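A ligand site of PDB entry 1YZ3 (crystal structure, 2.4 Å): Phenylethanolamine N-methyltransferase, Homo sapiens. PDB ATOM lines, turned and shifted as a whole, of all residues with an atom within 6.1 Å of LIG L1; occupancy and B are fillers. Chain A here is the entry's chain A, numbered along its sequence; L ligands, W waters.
The side-chain carboxylate (OD2) of Asp 267 is in salt-bridge range of a nitrogen (N1) of LIG L1 (3.6 Å).
OH of Tyr 85 sits at hydrogen-bond distance from O1 of LG2 L2 (2.9 Å).
A nitrogen (N1) of LIG L1 lies within salt-bridge range of the side-chain carboxylate (OE1) of Glu 219, 2.8 Å away.
OH of Tyr 40 lies within hydrogen-bond range of O2 of LG2 L2 (2.7 Å).
O2 of LG2 L2 is in hydrogen-bond range of OH of Tyr 35 (2.6 Å).
ND2 of Asn 39 sits at hydrogen-bond distance from O of Tyr 35.
The side-chain hydroxyl (OH) of Tyr 40 sits at hydrogen-bond distance from the side-chain amino group (NZ) of Lys 57, 3.4 Å away.
The side-chain amino group (NZ) of Lys 57 lies within hydrogen-bond range of the side-chain hydroxyl (OH) of Tyr 85, 3.3 Å away.
The side-chain carboxylate (OD2) of Asp 267 lies within salt-bridge range of the guanidinium group (NH1) of Arg 44, 2.9 Å away.
NH1 of Arg 44 is in hydrogen-bond range of OD1 of Asn 39.
The side-chain carboxylate of Asp 267 sits close to the backbone NH of Val 269.
The side-chain hydroxyl (OH) of Tyr 85 sits close to the side-chain hydroxyl (OH) of Tyr 40, 3.3 Å away.
Water W2 lies within hydrogen-bond range of the side-chain carboxylate of Asp 267 (2.5 Å), a nitrogen (N1) of LIG L1 (2.7 Å) and the side-chain amide oxygen of Asn 39 (2.8 Å).
Water W1 bridges the side-chain carboxylate (OE2) of Glu 185 (2.7 Å) and the side-chain carboxylate (OE2) of Glu 219 (2.9 Å).
Residues that only touch LIG L1: Tyr 35 (3.4 Å), Asn 39 (3.7 Å), Tyr 40 (3.4 Å), Arg 44 (3.7 Å), Val 53 (3.4 Å), Lys 57 (3.5 Å), Phe 182 (3.6 Å), Tyr 222 (3.9 Å), Met 258 (3.6 Å), Val 269 (3.7 Å) and Val 272 (3.9 Å).
Hydrophobic or aromatic side chains that line LIG L1: Tyr 35, Tyr 40, Val 53, Phe 182, Tyr 222, Met 258, Val 269 and Val 272.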
ATOM      1  N   TYR A  35       8.310  -1.181 -22.905  1.00  0.00           N
ATOM      2  CA  TYR A  35       7.590  -2.308 -23.476  1.00  0.00           C
ATOM      3  C   TYR A  35       6.326  -1.809 -24.182  1.00  0.00           C
ATOM      4  O   TYR A  35       6.020  -2.240 -25.289  1.00  0.00           O
ATOM      5  CB  TYR A  35       7.191  -3.285 -22.374  1.00  0.00           C
ATOM      6  CG  TYR A  35       6.400  -4.464 -22.900  1.00  0.00           C
ATOM      7  CD1 TYR A  35       7.042  -5.543 -23.502  1.00  0.00           C
ATOM      8  CD2 TYR A  35       5.011  -4.488 -22.795  1.00  0.00           C
ATOM      9  CE1 TYR A  35       6.308  -6.631 -23.994  1.00  0.00           C
ATOM     10  CE2 TYR A  35       4.270  -5.569 -23.289  1.00  0.00           C
ATOM     11  CZ  TYR A  35       4.922  -6.619 -23.877  1.00  0.00           C
ATOM     12  OH  TYR A  35       4.196  -7.694 -24.354  1.00  0.00           O
ATOM     13  N   ASN A  39       5.705  -1.871 -28.320  1.00  0.00           N
ATOM     14  CA  ASN A  39       4.664  -2.716 -28.895  1.00  0.00           C
ATOM     15  C   ASN A  39       3.272  -2.166 -29.043  1.00  0.00           C
ATOM     16  O   ASN A  39       2.487  -2.709 -29.820  1.00  0.00           O
ATOM     17  CB  ASN A  39       4.581  -4.013 -28.102  1.00  0.00           C
ATOM     18  CG  ASN A  39       5.902  -4.725 -28.059  1.00  0.00           C
ATOM     19  OD1 ASN A  39       6.369  -5.235 -29.064  1.00  0.00           O
ATOM     20  ND2 ASN A  39       6.521  -4.758 -26.878  1.00  0.00           N
ATOM     21  N   TYR A  40       2.953  -1.119 -28.315  1.00  0.00           N
ATOM     22  CA  TYR A  40       1.605  -0.577 -28.408  1.00  0.00           C
ATOM     23  C   TYR A  40       1.536   0.896 -28.749  1.00  0.00           C
ATOM     24  O   TYR A  40       0.546   1.547 -28.472  1.00  0.00           O
ATOM     25  CB  TYR A  40       0.852  -0.896 -27.122  1.00  0.00           C
ATOM     26  CG  TYR A  40       0.825  -2.389 -26.892  1.00  0.00           C
ATOM     27  CD1 TYR A  40       1.870  -3.036 -26.230  1.00  0.00           C
ATOM     28  CD2 TYR A  40      -0.201  -3.163 -27.430  1.00  0.00           C
ATOM     29  CE1 TYR A  40       1.889  -4.428 -26.106  1.00  0.00           C
ATOM     30  CE2 TYR A  40      -0.187  -4.547 -27.309  1.00  0.00           C
ATOM     31  CZ  TYR A  40       0.862  -5.181 -26.656  1.00  0.00           C
ATOM     32  OH  TYR A  40       0.867  -6.544 -26.564  1.00  0.00           O
ATOM     33  N   ARG A  44       3.274  -0.287 -34.611  1.00  0.00           N
ATOM     34  CA  ARG A  44       2.443  -1.407 -34.180  1.00  0.00           C
ATOM     35  C   ARG A  44       1.187  -0.957 -33.433  1.00  0.00           C
ATOM     36  O   ARG A  44       0.170  -1.644 -33.436  1.00  0.00           O
ATOM     37  CB  ARG A  44       3.231  -2.355 -33.282  1.00  0.00           C
ATOM     38  CG  ARG A  44       4.348  -3.082 -34.016  1.00  0.00           C
ATOM     39  CD  ARG A  44       5.138  -3.972 -33.087  1.00  0.00           C
ATOM     40  NE  ARG A  44       6.178  -4.696 -33.825  1.00  0.00           N
ATOM     41  CZ  ARG A  44       6.956  -5.619 -33.278  1.00  0.00           C
ATOM     42  NH1 ARG A  44       6.829  -5.929 -32.000  1.00  0.00           N
ATOM     43  NH2 ARG A  44       7.854  -6.245 -34.024  1.00  0.00           N
ATOM     44  N   VAL A  53      -0.947  -5.580 -36.853  1.00  0.00           N
ATOM     45  CA  VAL A  53      -1.088  -6.590 -35.813  1.00  0.00           C
ATOM     46  C   VAL A  53      -2.118  -6.204 -34.742  1.00  0.00           C
ATOM     47  O   VAL A  53      -2.831  -7.065 -34.232  1.00  0.00           O
ATOM     48  CB  VAL A  53       0.289  -6.890 -35.152  1.00  0.00           C
ATOM     49  CG1 VAL A  53       0.811  -5.665 -34.425  1.00  0.00           C
ATOM     50  CG2 VAL A  53       0.172  -8.089 -34.202  1.00  0.00           C
ATOM     51  N   GLY A  54      -2.189  -4.916 -34.396  1.00  0.00           N
ATOM     52  CA  GLY A  54      -3.159  -4.470 -33.398  1.00  0.00           C
ATOM     53  C   GLY A  54      -4.560  -4.884 -33.791  1.00  0.00           C
ATOM     54  O   GLY A  54      -5.239  -5.598 -33.050  1.00  0.00           O
ATOM     55  N   LYS A  57      -5.155  -8.818 -33.838  1.00  0.00           N
ATOM     56  CA  LYS A  57      -5.349  -9.415 -32.522  1.00  0.00           C
ATOM     57  C   LYS A  57      -6.753  -9.156 -31.982  1.00  0.00           C
ATOM     58  O   LYS A  57      -7.413 -10.077 -31.489  1.00  0.00           O
ATOM     59  CB  LYS A  57      -4.296  -8.885 -31.537  1.00  0.00           C
ATOM     60  CG  LYS A  57      -2.924  -9.547 -31.660  1.00  0.00           C
ATOM     61  CD  LYS A  57      -1.991  -9.162 -30.503  1.00  0.00           C
ATOM     62  CE  LYS A  57      -1.681  -7.674 -30.505  1.00  0.00           C
ATOM     63  NZ  LYS A  57      -0.642  -7.306 -29.518  1.00  0.00           N
ATOM     64  N   TYR A  85      -5.570  -4.440 -23.442  1.00  0.00           N
ATOM     65  CA  TYR A  85      -6.229  -4.678 -24.718  1.00  0.00           C
ATOM     66  C   TYR A  85      -6.773  -6.104 -24.878  1.00  0.00           C
ATOM     67  O   TYR A  85      -7.844  -6.303 -25.466  1.00  0.00           O
ATOM     68  CB  TYR A  85      -5.251  -4.399 -25.871  1.00  0.00           C
ATOM     69  CG  TYR A  85      -4.270  -5.523 -26.106  1.00  0.00           C
ATOM     70  CD1 TYR A  85      -4.597  -6.582 -26.946  1.00  0.00           C
ATOM     71  CD2 TYR A  85      -3.042  -5.555 -25.463  1.00  0.00           C
ATOM     72  CE1 TYR A  85      -3.740  -7.636 -27.133  1.00  0.00           C
ATOM     73  CE2 TYR A  85      -2.172  -6.609 -25.644  1.00  0.00           C
ATOM     74  CZ  TYR A  85      -2.526  -7.646 -26.476  1.00  0.00           C
ATOM     75  OH  TYR A  85      -1.658  -8.694 -26.670  1.00  0.00           O
ATOM     76  N   PHE A 182       1.336 -13.434 -25.200  1.00  0.00           N
ATOM     77  CA  PHE A 182       2.782 -13.238 -25.152  1.00  0.00           C
ATOM     78  C   PHE A 182       3.430 -13.501 -23.800  1.00  0.00           C
ATOM     79  O   PHE A 182       4.340 -12.783 -23.383  1.00  0.00           O
ATOM     80  CB  PHE A 182       3.146 -11.823 -25.626  1.00  0.00           C
ATOM     81  CG  PHE A 182       2.584 -11.471 -26.973  1.00  0.00           C
ATOM     82  CD1 PHE A 182       1.418 -10.718 -27.088  1.00  0.00           C
ATOM     83  CD2 PHE A 182       3.222 -11.901 -28.144  1.00  0.00           C
ATOM     84  CE1 PHE A 182       0.895 -10.387 -28.338  1.00  0.00           C
ATOM     85  CE2 PHE A 182       2.709 -11.578 -29.400  1.00  0.00           C
ATOM     86  CZ  PHE A 182       1.545 -10.817 -29.503  1.00  0.00           C
ATOM     87  N   GLU A 185       5.640 -18.361 -24.119  1.00  0.00           N
ATOM     88  CA  GLU A 185       6.837 -18.463 -24.934  1.00  0.00           C
ATOM     89  C   GLU A 185       7.892 -17.441 -24.540  1.00  0.00           C
ATOM     90  O   GLU A 185       9.083 -17.626 -24.798  1.00  0.00           O
ATOM     91  CB  GLU A 185       6.506 -18.317 -26.427  1.00  0.00           C
ATOM     92  CG  GLU A 185       6.248 -16.892 -26.947  1.00  0.00           C
ATOM     93  CD  GLU A 185       4.828 -16.371 -26.683  1.00  0.00           C
ATOM     94  OE1 GLU A 185       3.885 -17.200 -26.588  1.00  0.00           O
ATOM     95  OE2 GLU A 185       4.658 -15.137 -26.605  1.00  0.00           O
ATOM     96  N   ALA A 186       7.457 -16.362 -23.893  1.00  0.00           N
ATOM     97  CA  ALA A 186       8.379 -15.313 -23.497  1.00  0.00           C
ATOM     98  C   ALA A 186       9.046 -15.484 -22.130  1.00  0.00           C
ATOM     99  O   ALA A 186       9.947 -14.732 -21.774  1.00  0.00           O
ATOM    100  CB  ALA A 186       7.665 -13.961 -23.556  1.00  0.00           C
ATOM    101  N   ALA A 216       3.916 -15.026 -29.631  1.00  0.00           N
ATOM    102  CA  ALA A 216       4.887 -14.737 -30.687  1.00  0.00           C
ATOM    103  C   ALA A 216       5.326 -16.023 -31.400  1.00  0.00           C
ATOM    104  O   ALA A 216       5.509 -17.060 -30.769  1.00  0.00           O
ATOM    105  CB  ALA A 216       6.106 -14.041 -30.097  1.00  0.00           C
ATOM    106  N   GLU A 219      10.133 -16.327 -32.466  1.00  0.00           N
ATOM    107  CA  GLU A 219      10.866 -15.187 -31.922  1.00  0.00           C
ATOM    108  C   GLU A 219      11.880 -15.752 -30.934  1.00  0.00           C
ATOM    109  O   GLU A 219      11.581 -16.717 -30.229  1.00  0.00           O
ATOM    110  CB  GLU A 219       9.898 -14.233 -31.205  1.00  0.00           C
ATOM    111  CG  GLU A 219      10.551 -13.296 -30.200  1.00  0.00           C
ATOM    112  CD  GLU A 219       9.555 -12.349 -29.541  1.00  0.00           C
ATOM    113  OE1 GLU A 219       9.393 -11.217 -30.033  1.00  0.00           O
ATOM    114  OE2 GLU A 219       8.928 -12.746 -28.534  1.00  0.00           O
ATOM    115  N   TRP A 221      14.253 -13.266 -29.238  1.00  0.00           N
ATOM    116  CA  TRP A 221      14.557 -12.181 -28.299  1.00  0.00           C
ATOM    117  C   TRP A 221      13.680 -10.948 -28.530  1.00  0.00           C
ATOM    118  O   TRP A 221      13.130 -10.759 -29.620  1.00  0.00           O
ATOM    119  CB  TRP A 221      16.015 -11.736 -28.425  1.00  0.00           C
ATOM    120  CG  TRP A 221      16.336 -11.160 -29.778  1.00  0.00           C
ATOM    121  CD1 TRP A 221      16.755 -11.841 -30.887  1.00  0.00           C
ATOM    122  CD2 TRP A 221      16.243  -9.773 -30.171  1.00  0.00           C
ATOM    123  NE1 TRP A 221      16.929 -10.973 -31.937  1.00  0.00           N
ATOM    124  CE2 TRP A 221      16.622  -9.702 -31.526  1.00  0.00           C
ATOM    125  CE3 TRP A 221      15.873  -8.591 -29.509  1.00  0.00           C
ATOM    126  CZ2 TRP A 221      16.638  -8.492 -32.236  1.00  0.00           C
ATOM    127  CZ3 TRP A 221      15.889  -7.395 -30.217  1.00  0.00           C
ATOM    128  CH2 TRP A 221      16.267  -7.352 -31.572  1.00  0.00           C
ATOM    129  N   TYR A 222      13.565 -10.105 -27.505  1.00  0.00           N
ATOM    130  CA  TYR A 222      12.812  -8.845 -27.600  1.00  0.00           C
ATOM    131  C   TYR A 222      13.275  -7.938 -26.464  1.00  0.00           C
ATOM    132  O   TYR A 222      13.657  -8.410 -25.386  1.00  0.00           O
ATOM    133  CB  TYR A 222      11.294  -9.091 -27.535  1.00  0.00           C
ATOM    134  CG  TYR A 222      10.732  -9.401 -26.156  1.00  0.00           C
ATOM    135  CD1 TYR A 222      10.354  -8.368 -25.290  1.00  0.00           C
ATOM    136  CD2 TYR A 222      10.511 -10.711 -25.742  1.00  0.00           C
ATOM    137  CE1 TYR A 222       9.760  -8.632 -24.052  1.00  0.00           C
ATOM    138  CE2 TYR A 222       9.921 -10.996 -24.500  1.00  0.00           C
ATOM    139  CZ  TYR A 222       9.551  -9.943 -23.665  1.00  0.00           C
ATOM    140  OH  TYR A 222       8.934 -10.186 -22.461  1.00  0.00           O
ATOM    141  N   MET A 258       4.281 -11.317 -39.812  1.00  0.00           N
ATOM    142  CA  MET A 258       4.747  -9.950 -39.610  1.00  0.00           C
ATOM    143  C   MET A 258       5.121  -9.175 -40.869  1.00  0.00           C
ATOM    144  O   MET A 258       6.005  -9.567 -41.622  1.00  0.00           O
ATOM    145  CB  MET A 258       5.939  -9.929 -38.664  1.00  0.00           C
ATOM    146  CG  MET A 258       5.601  -9.786 -37.189  1.00  0.00           C
ATOM    147  SD  MET A 258       4.803  -8.210 -36.754  1.00  0.00           S
ATOM    148  CE  MET A 258       3.656  -8.784 -35.546  1.00  0.00           C
ATOM    149  N   ASP A 267      12.672  -6.496 -31.670  1.00  0.00           N
ATOM    150  CA  ASP A 267      12.655  -7.943 -31.539  1.00  0.00           C
ATOM    151  C   ASP A 267      12.901  -8.603 -32.889  1.00  0.00           C
ATOM    152  O   ASP A 267      13.232  -7.923 -33.853  1.00  0.00           O
ATOM    153  CB  ASP A 267      11.321  -8.437 -30.960  1.00  0.00           C
ATOM    154  CG  ASP A 267      10.114  -8.022 -31.801  1.00  0.00           C
ATOM    155  OD1 ASP A 267      10.168  -8.132 -33.049  1.00  0.00           O
ATOM    156  OD2 ASP A 267       9.094  -7.608 -31.205  1.00  0.00           O
ATOM    157  N   VAL A 269      10.538 -11.121 -33.977  1.00  0.00           N
ATOM    158  CA  VAL A 269       9.309 -11.896 -34.146  1.00  0.00           C
ATOM    159  C   VAL A 269       9.036 -12.106 -35.648  1.00  0.00           C
ATOM    160  O   VAL A 269       9.196 -11.174 -36.441  1.00  0.00           O
ATOM    161  CB  VAL A 269       8.108 -11.182 -33.497  1.00  0.00           C
ATOM    162  CG1 VAL A 269       7.869  -9.833 -34.192  1.00  0.00           C
ATOM    163  CG2 VAL A 269       6.863 -12.045 -33.558  1.00  0.00           C
ATOM    164  N   GLY A 271       6.054 -13.839 -36.665  1.00  0.00           N
ATOM    165  CA  GLY A 271       4.609 -13.825 -36.800  1.00  0.00           C
ATOM    166  C   GLY A 271       3.928 -13.834 -35.450  1.00  0.00           C
ATOM    167  O   GLY A 271       4.579 -13.710 -34.406  1.00  0.00           O
ATOM    168  N   VAL A 272       2.599 -13.963 -35.444  1.00  0.00           N
ATOM    169  CA  VAL A 272       1.841 -14.000 -34.196  1.00  0.00           C
ATOM    170  C   VAL A 272       0.733 -15.034 -34.338  1.00  0.00           C
ATOM    171  O   VAL A 272       0.088 -15.131 -35.392  1.00  0.00           O
ATOM    172  CB  VAL A 272       1.189 -12.631 -33.847  1.00  0.00           C
ATOM    173  CG1 VAL A 272       0.442 -12.745 -32.546  1.00  0.00           C
ATOM    174  CG2 VAL A 272       2.253 -11.539 -33.741  1.00  0.00           C
HETATM  175 CL1  LIG L   1       4.858  -9.101 -32.153  1.00  0.00          CL
HETATM  176  C1  LIG L   1       4.503  -8.599 -30.525  1.00  0.00           C
HETATM  177  C2  LIG L   1       5.365  -8.951 -29.488  1.00  0.00           C
HETATM  178  C3  LIG L   1       6.620  -9.797 -29.737  1.00  0.00           C
HETATM  179  N1  LIG L   1       7.571  -9.676 -28.613  1.00  0.00           N
HETATM  180  C4  LIG L   1       6.926 -10.007 -27.341  1.00  0.00           C
HETATM  181  C5  LIG L   1       5.935  -8.879 -26.989  1.00  0.00           C
HETATM  182  C6  LIG L   1       5.051  -8.552 -28.191  1.00  0.00           C
HETATM  183  C7  LIG L   1       3.903  -7.810 -27.941  1.00  0.00           C
HETATM  184  C8  LIG L   1       3.045  -7.458 -28.987  1.00  0.00           C
HETATM  185  C9  LIG L   1       3.349  -7.850 -30.278  1.00  0.00           C
HETATM  186 CL2  LIG L   1       2.266  -7.403 -31.550  1.00  0.00          CL
HETATM  187  N1  LG2 L   2       0.341 -10.017 -21.948  1.00  0.00           N
HETATM  188  C1  LG2 L   2       1.024  -8.750 -22.214  1.00  0.00           C
HETATM  189  C2  LG2 L   2       2.489  -8.818 -21.721  1.00  0.00           C
HETATM  190  C3  LG2 L   2       3.373  -9.935 -22.305  1.00  0.00           C
HETATM  191  S1  LG2 L   2       5.153  -9.733 -21.828  1.00  0.00           S
HETATM  192  C4  LG2 L   2       0.933  -8.373 -23.702  1.00  0.00           C
HETATM  193  O1  LG2 L   2       0.168  -9.043 -24.430  1.00  0.00           O
HETATM  194  O2  LG2 L   2       1.589  -7.394 -24.122  1.00  0.00           O
HETATM  195  C5  LG2 L   2       5.440 -11.244 -20.823  1.00  0.00           C
HETATM  196  C6  LG2 L   2       4.999 -11.027 -19.389  1.00  0.00           C
HETATM  197  O3  LG2 L   2       5.159 -12.220 -18.573  1.00  0.00           O
HETATM  198  C7  LG2 L   2       5.685  -9.886 -18.635  1.00  0.00           C
HETATM  199  O4  LG2 L   2       4.706  -8.967 -18.155  1.00  0.00           O
HETATM  200  C8  LG2 L   2       6.463 -10.601 -17.542  1.00  0.00           C
HETATM  201  O5  LG2 L   2       6.645  -9.851 -16.356  1.00  0.00           O
HETATM  202  C9  LG2 L   2       5.604 -11.839 -17.285  1.00  0.00           C
HETATM  203  N2  LG2 L   2       6.301 -12.954 -16.646  1.00  0.00           N
HETATM  204  C10 LG2 L   2       7.704 -13.104 -16.402  1.00  0.00           C
HETATM  205  N3  LG2 L   2       8.013 -14.217 -15.773  1.00  0.00           N
HETATM  206  C11 LG2 L   2       6.771 -14.833 -15.600  1.00  0.00           C
HETATM  207  C12 LG2 L   2       6.476 -16.076 -14.968  1.00  0.00           C
HETATM  208  N4  LG2 L   2       7.383 -16.876 -14.421  1.00  0.00           N
HETATM  209  N5  LG2 L   2       5.169 -16.452 -14.939  1.00  0.00           N
HETATM  210  C13 LG2 L   2       4.237 -15.637 -15.500  1.00  0.00           C
HETATM  211  N6  LG2 L   2       4.416 -14.438 -16.107  1.00  0.00           N
HETATM  212  C14 LG2 L   2       5.724 -14.096 -16.123  1.00  0.00           C
HETATM  213  O   HOH W   1       6.655 -13.274 -26.886  1.00  0.00           O
HETATM  214  O   HOH W   2       8.401  -7.076 -28.831  1.00  0.00           O
